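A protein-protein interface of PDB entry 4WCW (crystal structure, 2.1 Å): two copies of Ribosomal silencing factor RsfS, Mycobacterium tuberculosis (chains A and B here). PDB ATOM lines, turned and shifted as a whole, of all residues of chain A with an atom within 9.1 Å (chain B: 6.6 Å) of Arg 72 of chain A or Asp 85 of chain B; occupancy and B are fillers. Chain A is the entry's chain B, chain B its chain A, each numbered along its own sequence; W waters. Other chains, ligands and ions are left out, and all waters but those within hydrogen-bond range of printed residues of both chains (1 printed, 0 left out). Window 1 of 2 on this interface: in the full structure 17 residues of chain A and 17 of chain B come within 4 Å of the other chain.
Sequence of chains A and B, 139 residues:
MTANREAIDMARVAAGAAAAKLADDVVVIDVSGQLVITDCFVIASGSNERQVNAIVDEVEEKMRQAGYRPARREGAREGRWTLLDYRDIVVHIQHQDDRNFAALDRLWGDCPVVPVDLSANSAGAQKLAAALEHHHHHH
The backbone NH of Ile 37 of chain B sits at hydrogen-bond distance from the side-chain carboxylate of Glu 74 of chain A, at 2.9 Å.
OD2 of Asp 85 of chain A is in salt-bridge range of NE of Arg 72 of chain B (2.6 Å).
NH2 of Arg 72 of chain A sits at hydrogen-bond distance from OG1 of Thr 38 of chain B (2.7 Å).
OE1 of Glu 74 of chain A lies within hydrogen-bond range of OG1 of Thr 38 of chain B (2.7 Å).
The guanidinium group (NH2) of Arg 87 of chain A sits close to the guanidinium group (NH2) of Arg 87 of chain B (3.1 Å).
The side-chain carboxylate (OD2) of Asp 85 of chain B is in salt-bridge range of the guanidinium group (NE) of Arg 72 of chain A (2.6 Å).
The backbone carbonyl oxygen (O) of Arg 87 of chain B sits at hydrogen-bond distance from the guanidinium group (NH2) of Arg 72 of chain A (3.4 Å).
The backbone NH of Asp 85 of chain B is in hydrogen-bond range of the backbone carbonyl oxygen of Arg 72 of chain B.
The backbone carbonyl oxygen (O) of Arg 72 of chain A lies within hydrogen-bond range of the backbone NH (N) of Asp 85 of chain A (2.8 Å).
The guanidinium group (NH1) of Arg 72 of chain B is in salt-bridge range of the side-chain carboxylate (OE1) of Glu 74 of chain B, 3.1 Å away.
CG2 of Ile 37 of chain B touches NH1 of Arg 72 of chain A, at 3.7 Å.
Arg 72 of chain A touches Val 90 of chain B.
Arg 73 of chain A touches Ile 37 of chain B.
Arg 72 of chain B touches Arg 87 of chain A.
Val 90 of chain A touches Arg 72 of chain B.
Printed residues of chain B within 4 Å of Arg 72 of chain A: Ile 37 (3.7 Å), Thr 38 (2.7 Å), Asp 85 (2.6 Å), Arg 87 (3.4 Å) and Val 90 (3.5 Å).
Of the printed residues of chain A, Asp 85 of chain B touches Arg 72.
No residue of chain A comes within 4 Å of Ala 71 of chain B.
Of the printed residues of chain A, Arg 72 of chain B touches Asp 85, Arg 87 and Val 90.
Printed residues of chain B within 4 Å of Val 90 of chain A: Arg 72 (3.8 Å).
Of the printed residues of chain A, Thr 38 of chain B touches Arg 72 (2.7 Å) and Glu 74 (2.7 Å).
The nearest residue of chain A that does not touch Asp 85 of chain B is Asp 85 of chain A (4.8 Å).
The nearest printed residue of chain B that does not touch Glu 74 of chain A is Arg 87 of chain B (5.0 Å).
Of the 17 printed residues of chain B, 6 touch a printed residue of chain A.
Printed residues of chain B that touch a printed residue of chain A: Ile 37, Thr 38, Arg 72, Asp 85, Arg 87 and Val 90.
Hydrophobic or aromatic side chains of chain B within 4 Å of the printed part of chain A: Ile 37 and Val 90.
Of the 17 printed residues of chain A, 6 touch a printed residue of chain B.
Printed residues of chain A that touch a printed residue of chain B: Arg 72, Arg 73, Glu 74, Asp 85, Arg 87 and Val 90.
Hydrophobic or aromatic side chains of chain A within 4 Å of the printed part of chain B: Val 90.
Among the printed residues, 12 pairs touch across the chains.
Among the printed residues, Asp or Glu carboxylates within 4 Å of a Lys or Arg side-chain nitrogen of the other chain: Arg 72 of chain A with Asp 85 of chain B (2.6 Å) and Asp 85 of chain A with Arg 72 of chain B (2.6 Å).
Arg 72 of chain A touches Asp 85 of chain B, and with the chains exchanged Asp 85 of chain A touches Arg 72 of chain B.
Arg 72 of chain A touches Val 90 of chain B, and with the chains exchanged Val 90 of chain A touches Arg 72 of chain B.
Positions printed for both chains: 69, 70, 71, 72, 73, 74, 83, 84, 85, 86, 87, 89, 90 and 91.
Of the 12 pairs that touch across the chains among the printed residues, 7 have their exchanged pair printed and touching as well.
Water W1 lies within hydrogen-bond range of the side-chain carboxylate (OD2) of Asp 85 of chain A (2.6 Å) and the side-chain carboxylate (OD2) of Asp 85 of chain B (2.9 Å).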
ATOM      1  N   ARG A  69     -24.665   1.780  16.490  1.00  0.00           N
ATOM      2  CA  ARG A  69     -25.002   0.405  16.159  1.00  0.00           C
ATOM      3  C   ARG A  69     -23.822  -0.307  15.512  1.00  0.00           C
ATOM      4  O   ARG A  69     -23.025   0.316  14.809  1.00  0.00           O
ATOM      5  CB  ARG A  69     -26.183   0.411  15.191  1.00  0.00           C
ATOM      6  CG  ARG A  69     -25.963   1.350  14.021  1.00  0.00           C
ATOM      7  CD  ARG A  69     -27.070   1.272  12.999  1.00  0.00           C
ATOM      8  NE  ARG A  69     -28.257   2.021  13.399  1.00  0.00           N
ATOM      9  CZ  ARG A  69     -28.453   3.307  13.123  1.00  0.00           C
ATOM     10  NH1 ARG A  69     -27.533   3.990  12.455  1.00  0.00           N
ATOM     11  NH2 ARG A  69     -29.565   3.912  13.520  1.00  0.00           N
ATOM     12  N   PRO A  70     -23.691  -1.617  15.767  1.00  0.00           N
ATOM     13  CA  PRO A  70     -22.628  -2.386  15.119  1.00  0.00           C
ATOM     14  C   PRO A  70     -22.904  -2.416  13.627  1.00  0.00           C
ATOM     15  O   PRO A  70     -24.069  -2.372  13.225  1.00  0.00           O
ATOM     16  CB  PRO A  70     -22.787  -3.791  15.719  1.00  0.00           C
ATOM     17  CG  PRO A  70     -23.610  -3.604  16.970  1.00  0.00           C
ATOM     18  CD  PRO A  70     -24.506  -2.438  16.679  1.00  0.00           C
ATOM     19  N   ALA A  71     -21.859  -2.468  12.813  1.00  0.00           N
ATOM     20  CA  ALA A  71     -22.051  -2.576  11.367  1.00  0.00           C
ATOM     21  C   ALA A  71     -22.490  -3.970  10.930  1.00  0.00           C
ATOM     22  O   ALA A  71     -22.068  -4.977  11.508  1.00  0.00           O
ATOM     23  CB  ALA A  71     -20.780  -2.188  10.632  1.00  0.00           C
ATOM     24  N   ARG A  72     -23.343  -4.023   9.911  1.00  0.00           N
ATOM     25  CA  ARG A  72     -23.550  -5.257   9.164  1.00  0.00           C
ATOM     26  C   ARG A  72     -22.374  -5.300   8.203  1.00  0.00           C
ATOM     27  O   ARG A  72     -22.324  -4.530   7.242  1.00  0.00           O
ATOM     28  CB  ARG A  72     -24.883  -5.214   8.399  1.00  0.00           C
ATOM     29  CG  ARG A  72     -25.367  -6.545   7.777  1.00  0.00           C
ATOM     30  CD  ARG A  72     -24.519  -7.016   6.587  1.00  0.00           C
ATOM     31  NE  ARG A  72     -25.267  -7.834   5.630  1.00  0.00           N
ATOM     32  CZ  ARG A  72     -24.701  -8.660   4.755  1.00  0.00           C
ATOM     33  NH1 ARG A  72     -23.384  -8.800   4.732  1.00  0.00           N
ATOM     34  NH2 ARG A  72     -25.447  -9.358   3.910  1.00  0.00           N
ATOM     35  N   ARG A  73     -21.417  -6.182   8.466  1.00  0.00           N
ATOM     36  CA  ARG A  73     -20.222  -6.256   7.635  1.00  0.00           C
ATOM     37  C   ARG A  73     -20.371  -7.211   6.467  1.00  0.00           C
ATOM     38  O   ARG A  73     -21.192  -8.134   6.487  1.00  0.00           O
ATOM     39  CB  ARG A  73     -19.003  -6.658   8.473  1.00  0.00           C
ATOM     40  CG  ARG A  73     -19.024  -8.087   8.980  1.00  0.00           C
ATOM     41  CD  ARG A  73     -17.854  -8.343   9.933  1.00  0.00           C
ATOM     42  NE  ARG A  73     -17.861  -9.711  10.444  1.00  0.00           N
ATOM     43  CZ  ARG A  73     -17.180 -10.716   9.902  1.00  0.00           C
ATOM     44  NH1 ARG A  73     -16.435 -10.511   8.823  1.00  0.00           N
ATOM     45  NH2 ARG A  73     -17.238 -11.929  10.439  1.00  0.00           N
ATOM     46  N   GLU A  74     -19.581  -6.958   5.431  1.00  0.00           N
ATOM     47  CA  GLU A  74     -19.438  -7.892   4.327  1.00  0.00           C
ATOM     48  C   GLU A  74     -18.024  -7.746   3.812  1.00  0.00           C
ATOM     49  O   GLU A  74     -17.386  -6.722   4.050  1.00  0.00           O
ATOM     50  CB  GLU A  74     -20.447  -7.592   3.220  1.00  0.00           C
ATOM     51  CG  GLU A  74     -20.531  -8.672   2.142  1.00  0.00           C
ATOM     52  CD  GLU A  74     -20.686 -10.064   2.726  1.00  0.00           C
ATOM     53  OE1 GLU A  74     -21.834 -10.543   2.848  1.00  0.00           O
ATOM     54  OE2 GLU A  74     -19.659 -10.688   3.066  1.00  0.00           O
ATOM     55  N   GLY A  75     -17.514  -8.759   3.125  1.00  0.00           N
ATOM     56  CA  GLY A  75     -16.181  -8.643   2.567  1.00  0.00           C
ATOM     57  C   GLY A  75     -15.833  -9.701   1.546  1.00  0.00           C
ATOM     58  O   GLY A  75     -16.444 -10.775   1.504  1.00  0.00           O
ATOM     59  N   TRP A  81     -11.656  -6.127  -0.505  1.00  0.00           N
ATOM     60  CA  TRP A  81     -12.561  -5.077  -0.059  1.00  0.00           C
ATOM     61  C   TRP A  81     -13.368  -5.525   1.148  1.00  0.00           C
ATOM     62  O   TRP A  81     -13.603  -6.721   1.348  1.00  0.00           O
ATOM     63  CB  TRP A  81     -13.492  -4.640  -1.192  1.00  0.00           C
ATOM     64  CG  TRP A  81     -14.405  -5.710  -1.694  1.00  0.00           C
ATOM     65  CD1 TRP A  81     -14.185  -6.555  -2.744  1.00  0.00           C
ATOM     66  CD2 TRP A  81     -15.699  -6.047  -1.176  1.00  0.00           C
ATOM     67  NE1 TRP A  81     -15.259  -7.395  -2.910  1.00  0.00           N
ATOM     68  CE2 TRP A  81     -16.201  -7.102  -1.957  1.00  0.00           C
ATOM     69  CE3 TRP A  81     -16.477  -5.551  -0.123  1.00  0.00           C
ATOM     70  CZ2 TRP A  81     -17.452  -7.678  -1.719  1.00  0.00           C
ATOM     71  CZ3 TRP A  81     -17.711  -6.124   0.113  1.00  0.00           C
ATOM     72  CH2 TRP A  81     -18.187  -7.174  -0.679  1.00  0.00           C
ATOM     73  N   THR A  82     -13.777  -4.555   1.957  1.00  0.00           N
ATOM     74  CA  THR A  82     -14.669  -4.803   3.081  1.00  0.00           C
ATOM     75  C   THR A  82     -15.706  -3.687   3.144  1.00  0.00           C
ATOM     76  O   THR A  82     -15.401  -2.515   2.893  1.00  0.00           O
ATOM     77  CB  THR A  82     -13.911  -4.914   4.433  1.00  0.00           C
ATOM     78  OG1 THR A  82     -13.160  -6.134   4.468  1.00  0.00           O
ATOM     79  CG2 THR A  82     -14.891  -4.933   5.597  1.00  0.00           C
ATOM     80  N   LEU A  83     -16.940  -4.055   3.457  1.00  0.00           N
ATOM     81  CA  LEU A  83     -18.014  -3.076   3.554  1.00  0.00           C
ATOM     82  C   LEU A  83     -18.642  -3.120   4.941  1.00  0.00           C
ATOM     83  O   LEU A  83     -18.868  -4.201   5.491  1.00  0.00           O
ATOM     84  CB  LEU A  83     -19.061  -3.356   2.472  1.00  0.00           C
ATOM     85  CG  LEU A  83     -20.197  -2.355   2.263  1.00  0.00           C
ATOM     86  CD1 LEU A  83     -20.279  -1.948   0.812  1.00  0.00           C
ATOM     87  CD2 LEU A  83     -21.517  -2.942   2.730  1.00  0.00           C
ATOM     88  N   LEU A  84     -18.916  -1.949   5.513  1.00  0.00           N
ATOM     89  CA  LEU A  84     -19.615  -1.873   6.794  1.00  0.00           C
ATOM     90  C   LEU A  84     -20.914  -1.093   6.630  1.00  0.00           C
ATOM     91  O   LEU A  84     -20.889   0.097   6.317  1.00  0.00           O
ATOM     92  CB  LEU A  84     -18.741  -1.199   7.856  1.00  0.00           C
ATOM     93  CG  LEU A  84     -17.377  -1.802   8.201  1.00  0.00           C
ATOM     94  CD1 LEU A  84     -16.591  -0.868   9.121  1.00  0.00           C
ATOM     95  CD2 LEU A  84     -17.531  -3.178   8.839  1.00  0.00           C
ATOM     96  N   ASP A  85     -22.045  -1.762   6.833  1.00  0.00           N
ATOM     97  CA  ASP A  85     -23.353  -1.120   6.699  1.00  0.00           C
ATOM     98  C   ASP A  85     -23.865  -0.649   8.056  1.00  0.00           C
ATOM     99  O   ASP A  85     -24.150  -1.461   8.935  1.00  0.00           O
ATOM    100  CB  ASP A  85     -24.356  -2.084   6.054  1.00  0.00           C
ATOM    101  CG  ASP A  85     -25.736  -1.472   5.887  1.00  0.00           C
ATOM    102  OD1 ASP A  85     -25.844  -0.227   5.850  1.00  0.00           O
ATOM    103  OD2 ASP A  85     -26.720  -2.233   5.784  1.00  0.00           O
ATOM    104  N   TYR A  86     -23.966   0.666   8.221  1.00  0.00           N
ATOM    105  CA  TYR A  86     -24.519   1.259   9.432  1.00  0.00           C
ATOM    106  C   TYR A  86     -25.935   1.793   9.184  1.00  0.00           C
ATOM    107  O   TYR A  86     -26.475   2.534  10.012  1.00  0.00           O
ATOM    108  CB  TYR A  86     -23.609   2.392   9.933  1.00  0.00           C
ATOM    109  CG  TYR A  86     -22.256   1.931  10.426  1.00  0.00           C
ATOM    110  CD1 TYR A  86     -22.094   1.431  11.711  1.00  0.00           C
ATOM    111  CD2 TYR A  86     -21.143   1.995   9.604  1.00  0.00           C
ATOM    112  CE1 TYR A  86     -20.859   1.006  12.154  1.00  0.00           C
ATOM    113  CE2 TYR A  86     -19.914   1.573  10.035  1.00  0.00           C
ATOM    114  CZ  TYR A  86     -19.776   1.078  11.306  1.00  0.00           C
ATOM    115  OH  TYR A  86     -18.537   0.662  11.728  1.00  0.00           O
ATOM    116  N   ARG A  87     -26.520   1.385   8.055  1.00  0.00           N
ATOM    117  CA  ARG A  87     -27.814   1.874   7.545  1.00  0.00           C
ATOM    118  C   ARG A  87     -27.742   3.320   7.068  1.00  0.00           C
ATOM    119  O   ARG A  87     -27.867   3.593   5.875  1.00  0.00           O
ATOM    120  CB  ARG A  87     -28.970   1.710   8.545  1.00  0.00           C
ATOM    121  CG  ARG A  87     -29.306   0.282   8.916  1.00  0.00           C
ATOM    122  CD  ARG A  87     -28.678  -0.073  10.252  1.00  0.00           C
ATOM    123  NE  ARG A  87     -29.087  -1.385  10.745  1.00  0.00           N
ATOM    124  CZ  ARG A  87     -28.366  -2.491  10.598  1.00  0.00           C
ATOM    125  NH1 ARG A  87     -27.197  -2.442   9.972  1.00  0.00           N
ATOM    126  NH2 ARG A  87     -28.811  -3.642  11.079  1.00  0.00           N
ATOM    127  N   ILE A  89     -25.189   5.265   7.016  1.00  0.00           N
ATOM    128  CA  ILE A  89     -24.063   5.307   6.085  1.00  0.00           C
ATOM    129  C   ILE A  89     -23.572   3.904   5.764  1.00  0.00           C
ATOM    130  O   ILE A  89     -23.804   2.962   6.522  1.00  0.00           O
ATOM    131  CB  ILE A  89     -22.864   6.151   6.596  1.00  0.00           C
ATOM    132  CG1 ILE A  89     -22.106   5.417   7.704  1.00  0.00           C
ATOM    133  CG2 ILE A  89     -23.311   7.544   7.056  1.00  0.00           C
ATOM    134  CD1 ILE A  89     -20.764   6.044   8.025  1.00  0.00           C
ATOM    135  N   VAL A  90     -22.903   3.777   4.626  1.00  0.00           N
ATOM    136  CA  VAL A  90     -22.223   2.542   4.262  1.00  0.00           C
ATOM    137  C   VAL A  90     -20.748   2.867   4.058  1.00  0.00           C
ATOM    138  O   VAL A  90     -20.412   3.828   3.359  1.00  0.00           O
ATOM    139  CB  VAL A  90     -22.796   1.945   2.962  1.00  0.00           C
ATOM    140  CG1 VAL A  90     -21.976   0.746   2.524  1.00  0.00           C
ATOM    141  CG2 VAL A  90     -24.247   1.554   3.145  1.00  0.00           C
ATOM    142  N   VAL A  91     -19.866   2.094   4.686  1.00  0.00           N
ATOM    143  CA  VAL A  91     -18.435   2.342   4.550  1.00  0.00           C
ATOM    144  C   VAL A  91     -17.840   1.302   3.620  1.00  0.00           C
ATOM    145  O   VAL A  91     -18.059   0.106   3.812  1.00  0.00           O
ATOM    146  CB  VAL A  91     -17.716   2.296   5.913  1.00  0.00           C
ATOM    147  CG1 VAL A  91     -16.211   2.435   5.731  1.00  0.00           C
ATOM    148  CG2 VAL A  91     -18.243   3.386   6.830  1.00  0.00           C
ATOM    149  N   ILE B  37     -19.627 -13.129   4.662  1.00  0.00           N
ATOM    150  CA  ILE B  37     -20.857 -13.151   5.452  1.00  0.00           C
ATOM    151  C   ILE B  37     -22.039 -13.800   4.721  1.00  0.00           C
ATOM    152  O   ILE B  37     -22.555 -14.841   5.137  1.00  0.00           O
ATOM    153  CB  ILE B  37     -21.261 -11.743   5.906  1.00  0.00           C
ATOM    154  CG1 ILE B  37     -20.151 -11.107   6.744  1.00  0.00           C
ATOM    155  CG2 ILE B  37     -22.546 -11.805   6.709  1.00  0.00           C
ATOM    156  CD1 ILE B  37     -19.979 -11.742   8.114  1.00  0.00           C
ATOM    157  N   THR B  38     -22.483 -13.177   3.636  1.00  0.00           N
ATOM    158  CA  THR B  38     -23.631 -13.707   2.905  1.00  0.00           C
ATOM    159  C   THR B  38     -23.266 -15.005   2.195  1.00  0.00           C
ATOM    160  O   THR B  38     -22.188 -15.110   1.614  1.00  0.00           O
ATOM    161  CB  THR B  38     -24.163 -12.702   1.877  1.00  0.00           C
ATOM    162  OG1 THR B  38     -24.362 -11.430   2.510  1.00  0.00           O
ATOM    163  CG2 THR B  38     -25.485 -13.191   1.328  1.00  0.00           C
ATOM    164  N   ARG B  69     -36.254 -11.892  11.111  1.00  0.00           N
ATOM    165  CA  ARG B  69     -36.475 -10.474  11.377  1.00  0.00           C
ATOM    166  C   ARG B  69     -36.531  -9.762  10.030  1.00  0.00           C
ATOM    167  O   ARG B  69     -35.961 -10.259   9.057  1.00  0.00           O
ATOM    168  CB  ARG B  69     -35.336  -9.935  12.258  1.00  0.00           C
ATOM    169  CG  ARG B  69     -35.685  -8.723  13.132  1.00  0.00           C
ATOM    170  CD  ARG B  69     -34.802  -8.629  14.367  1.00  0.00           C
ATOM    171  NE  ARG B  69     -35.196  -9.600  15.387  1.00  0.00           N
ATOM    172  CZ  ARG B  69     -36.060  -9.347  16.367  1.00  0.00           C
ATOM    173  NH1 ARG B  69     -36.627  -8.152  16.466  1.00  0.00           N
ATOM    174  NH2 ARG B  69     -36.361 -10.290  17.250  1.00  0.00           N
ATOM    175  N   PRO B  70     -37.256  -8.628   9.951  1.00  0.00           N
ATOM    176  CA  PRO B  70     -37.347  -7.866   8.700  1.00  0.00           C
ATOM    177  C   PRO B  70     -35.989  -7.581   8.068  1.00  0.00           C
ATOM    178  O   PRO B  70     -35.029  -7.281   8.772  1.00  0.00           O
ATOM    179  CB  PRO B  70     -37.988  -6.549   9.148  1.00  0.00           C
ATOM    180  CG  PRO B  70     -38.876  -6.948  10.282  1.00  0.00           C
ATOM    181  CD  PRO B  70     -38.160  -8.084  10.984  1.00  0.00           C
ATOM    182  N   ALA B  71     -35.920  -7.675   6.747  1.00  0.00           N
ATOM    183  CA  ALA B  71     -34.686  -7.385   6.026  1.00  0.00           C
ATOM    184  C   ALA B  71     -34.269  -5.947   6.228  1.00  0.00           C
ATOM    185  O   ALA B  71     -35.110  -5.073   6.445  1.00  0.00           O
ATOM    186  CB  ALA B  71     -34.868  -7.651   4.544  1.00  0.00           C
ATOM    187  N   ARG B  72     -32.969  -5.700   6.160  1.00  0.00           N
ATOM    188  CA  ARG B  72     -32.493  -4.337   5.993  1.00  0.00           C
ATOM    189  C   ARG B  72     -32.743  -4.051   4.523  1.00  0.00           C
ATOM    190  O   ARG B  72     -32.312  -4.814   3.662  1.00  0.00           O
ATOM    191  CB  ARG B  72     -31.004  -4.234   6.342  1.00  0.00           C
ATOM    192  CG  ARG B  72     -30.418  -2.808   6.391  1.00  0.00           C
ATOM    193  CD  ARG B  72     -30.181  -2.203   5.001  1.00  0.00           C
ATOM    194  NE  ARG B  72     -29.002  -1.338   4.950  1.00  0.00           N
ATOM    195  CZ  ARG B  72     -28.895  -0.247   4.196  1.00  0.00           C
ATOM    196  NH1 ARG B  72     -29.902   0.142   3.429  1.00  0.00           N
ATOM    197  NH2 ARG B  72     -27.777   0.465   4.213  1.00  0.00           N
ATOM    198  N   ARG B  73     -33.459  -2.975   4.226  1.00  0.00           N
ATOM    199  CA  ARG B  73     -33.888  -2.738   2.856  1.00  0.00           C
ATOM    200  C   ARG B  73     -33.123  -1.607   2.185  1.00  0.00           C
ATOM    201  O   ARG B  73     -32.565  -0.732   2.853  1.00  0.00           O
ATOM    202  CB  ARG B  73     -35.391  -2.453   2.809  1.00  0.00           C
ATOM    203  CG  ARG B  73     -36.243  -3.651   3.133  1.00  0.00           C
ATOM    204  CD  ARG B  73     -37.691  -3.431   2.742  1.00  0.00           C
ATOM    205  NE  ARG B  73     -38.474  -2.867   3.836  1.00  0.00           N
ATOM    206  CZ  ARG B  73     -39.779  -2.631   3.773  1.00  0.00           C
ATOM    207  NH1 ARG B  73     -40.449  -2.912   2.664  1.00  0.00           N
ATOM    208  NH2 ARG B  73     -40.414  -2.113   4.814  1.00  0.00           N
ATOM    209  N   GLU B  74     -33.093  -1.647   0.858  1.00  0.00           N
ATOM    210  CA  GLU B  74     -32.575  -0.542   0.059  1.00  0.00           C
ATOM    211  C   GLU B  74     -33.196  -0.547  -1.334  1.00  0.00           C
ATOM    212  O   GLU B  74     -33.613  -1.597  -1.847  1.00  0.00           O
ATOM    213  CB  GLU B  74     -31.048  -0.592  -0.024  1.00  0.00           C
ATOM    214  CG  GLU B  74     -30.400   0.681  -0.566  1.00  0.00           C
ATOM    215  CD  GLU B  74     -30.742   1.913   0.252  1.00  0.00           C
ATOM    216  OE1 GLU B  74     -29.968   2.248   1.176  1.00  0.00           O
ATOM    217  OE2 GLU B  74     -31.781   2.557  -0.034  1.00  0.00           O
ATOM    218  N   LEU B  83     -33.618  -4.045  -2.617  1.00  0.00           N
ATOM    219  CA  LEU B  83     -32.645  -4.970  -2.067  1.00  0.00           C
ATOM    220  C   LEU B  83     -33.055  -5.369  -0.651  1.00  0.00           C
ATOM    221  O   LEU B  83     -33.287  -4.510   0.197  1.00  0.00           O
ATOM    222  CB  LEU B  83     -31.272  -4.310  -2.048  1.00  0.00           C
ATOM    223  CG  LEU B  83     -30.107  -5.165  -1.565  1.00  0.00           C
ATOM    224  CD1 LEU B  83     -29.794  -6.177  -2.625  1.00  0.00           C
ATOM    225  CD2 LEU B  83     -28.907  -4.283  -1.297  1.00  0.00           C
ATOM    226  N   LEU B  84     -33.151  -6.670  -0.400  1.00  0.00           N
ATOM    227  CA  LEU B  84     -33.497  -7.164   0.933  1.00  0.00           C
ATOM    228  C   LEU B  84     -32.318  -7.910   1.543  1.00  0.00           C
ATOM    229  O   LEU B  84     -31.943  -8.982   1.063  1.00  0.00           O
ATOM    230  CB  LEU B  84     -34.700  -8.106   0.857  1.00  0.00           C
ATOM    231  CG  LEU B  84     -35.994  -7.586   0.246  1.00  0.00           C
ATOM    232  CD1 LEU B  84     -37.039  -8.676   0.250  1.00  0.00           C
ATOM    233  CD2 LEU B  84     -36.492  -6.385   0.994  1.00  0.00           C
ATOM    234  N   ASP B  85     -31.738  -7.356   2.603  1.00  0.00           N
ATOM    235  CA  ASP B  85     -30.600  -7.996   3.255  1.00  0.00           C
ATOM    236  C   ASP B  85     -31.035  -8.759   4.503  1.00  0.00           C
ATOM    237  O   ASP B  85     -31.422  -8.147   5.500  1.00  0.00           O
ATOM    238  CB  ASP B  85     -29.546  -6.946   3.619  1.00  0.00           C
ATOM    239  CG  ASP B  85     -28.268  -7.558   4.159  1.00  0.00           C
ATOM    240  OD1 ASP B  85     -28.102  -8.793   4.078  1.00  0.00           O
ATOM    241  OD2 ASP B  85     -27.411  -6.794   4.646  1.00  0.00           O
ATOM    242  N   TYR B  86     -30.959 -10.088   4.438  1.00  0.00           N
ATOM    243  CA  TYR B  86     -31.220 -10.952   5.591  1.00  0.00           C
ATOM    244  C   TYR B  86     -29.916 -11.507   6.171  1.00  0.00           C
ATOM    245  O   TYR B  86     -29.933 -12.456   6.957  1.00  0.00           O
ATOM    246  CB  TYR B  86     -32.175 -12.100   5.223  1.00  0.00           C
ATOM    247  CG  TYR B  86     -33.565 -11.640   4.858  1.00  0.00           C
ATOM    248  CD1 TYR B  86     -34.532 -11.437   5.834  1.00  0.00           C
ATOM    249  CD2 TYR B  86     -33.909 -11.403   3.536  1.00  0.00           C
ATOM    250  CE1 TYR B  86     -35.806 -11.008   5.499  1.00  0.00           C
ATOM    251  CE2 TYR B  86     -35.172 -10.978   3.191  1.00  0.00           C
ATOM    252  CZ  TYR B  86     -36.112 -10.780   4.177  1.00  0.00           C
ATOM    253  OH  TYR B  86     -37.366 -10.349   3.820  1.00  0.00           O
ATOM    254  N   ARG B  87     -28.800 -10.893   5.776  1.00  0.00           N
ATOM    255  CA  ARG B  87     -27.441 -11.275   6.202  1.00  0.00           C
ATOM    256  C   ARG B  87     -26.910 -12.582   5.601  1.00  0.00           C
ATOM    257  O   ARG B  87     -25.988 -12.557   4.779  1.00  0.00           O
ATOM    258  CB  ARG B  87     -27.289 -11.230   7.729  1.00  0.00           C
ATOM    259  CG  ARG B  87     -27.616  -9.859   8.276  1.00  0.00           C
ATOM    260  CD  ARG B  87     -27.394  -9.717   9.763  1.00  0.00           C
ATOM    261  NE  ARG B  87     -27.856  -8.397  10.179  1.00  0.00           N
ATOM    262  CZ  ARG B  87     -27.547  -7.809  11.324  1.00  0.00           C
ATOM    263  NH1 ARG B  87     -26.762  -8.420  12.198  1.00  0.00           N
ATOM    264  NH2 ARG B  87     -28.027  -6.604  11.593  1.00  0.00           N
ATOM    265  N   ASP B  88     -27.485 -13.713   5.994  1.00  0.00           N
ATOM    266  CA  ASP B  88     -27.053 -14.998   5.437  1.00  0.00           C
ATOM    267  C   ASP B  88     -27.416 -15.068   3.965  1.00  0.00           C
ATOM    268  O   ASP B  88     -26.715 -15.687   3.155  1.00  0.00           O
ATOM    269  CB  ASP B  88     -27.695 -16.165   6.185  1.00  0.00           C
ATOM    270  CG  ASP B  88     -27.441 -16.113   7.679  1.00  0.00           C
ATOM    271  OD1 ASP B  88     -26.296 -16.371   8.112  1.00  0.00           O
ATOM    272  OD2 ASP B  88     -28.397 -15.834   8.426  1.00  0.00           O
ATOM    273  N   ILE B  89     -28.531 -14.429   3.624  1.00  0.00           N
ATOM    274  CA  ILE B  89     -28.918 -14.262   2.237  1.00  0.00           C
ATOM    275  C   ILE B  89     -29.249 -12.804   1.957  1.00  0.00           C
ATOM    276  O   ILE B  89     -29.567 -12.030   2.865  1.00  0.00           O
ATOM    277  CB  ILE B  89     -30.129 -15.129   1.852  1.00  0.00           C
ATOM    278  CG1 ILE B  89     -31.428 -14.519   2.388  1.00  0.00           C
ATOM    279  CG2 ILE B  89     -29.943 -16.550   2.340  1.00  0.00           C
ATOM    280  CD1 ILE B  89     -32.690 -15.194   1.844  1.00  0.00           C
ATOM    281  N   VAL B  90     -29.169 -12.434   0.688  1.00  0.00           N
ATOM    282  CA  VAL B  90     -29.559 -11.106   0.247  1.00  0.00           C
ATOM    283  C   VAL B  90     -30.442 -11.299  -0.963  1.00  0.00           C
ATOM    284  O   VAL B  90     -30.112 -12.095  -1.845  1.00  0.00           O
ATOM    285  CB  VAL B  90     -28.327 -10.290  -0.148  1.00  0.00           C
ATOM    286  CG1 VAL B  90     -28.726  -9.049  -0.927  1.00  0.00           C
ATOM    287  CG2 VAL B  90     -27.505  -9.941   1.086  1.00  0.00           C
ATOM    288  N   VAL B  91     -31.574 -10.598  -1.003  1.00  0.00           N
ATOM    289  CA  VAL B  91     -32.510 -10.749  -2.119  1.00  0.00           C
ATOM    290  C   VAL B  91     -32.528  -9.484  -2.973  1.00  0.00           C
ATOM    291  O   VAL B  91     -32.625  -8.371  -2.447  1.00  0.00           O
ATOM    292  CB  VAL B  91     -33.932 -11.078  -1.621  1.00  0.00           C
ATOM    293  CG1 VAL B  91     -34.859 -11.381  -2.794  1.00  0.00           C
ATOM    294  CG2 VAL B  91     -33.888 -12.262  -0.675  1.00  0.00           C
HETATM  295  O   HOH W   1     -27.535  -4.568   6.552  1.00  0.00           O
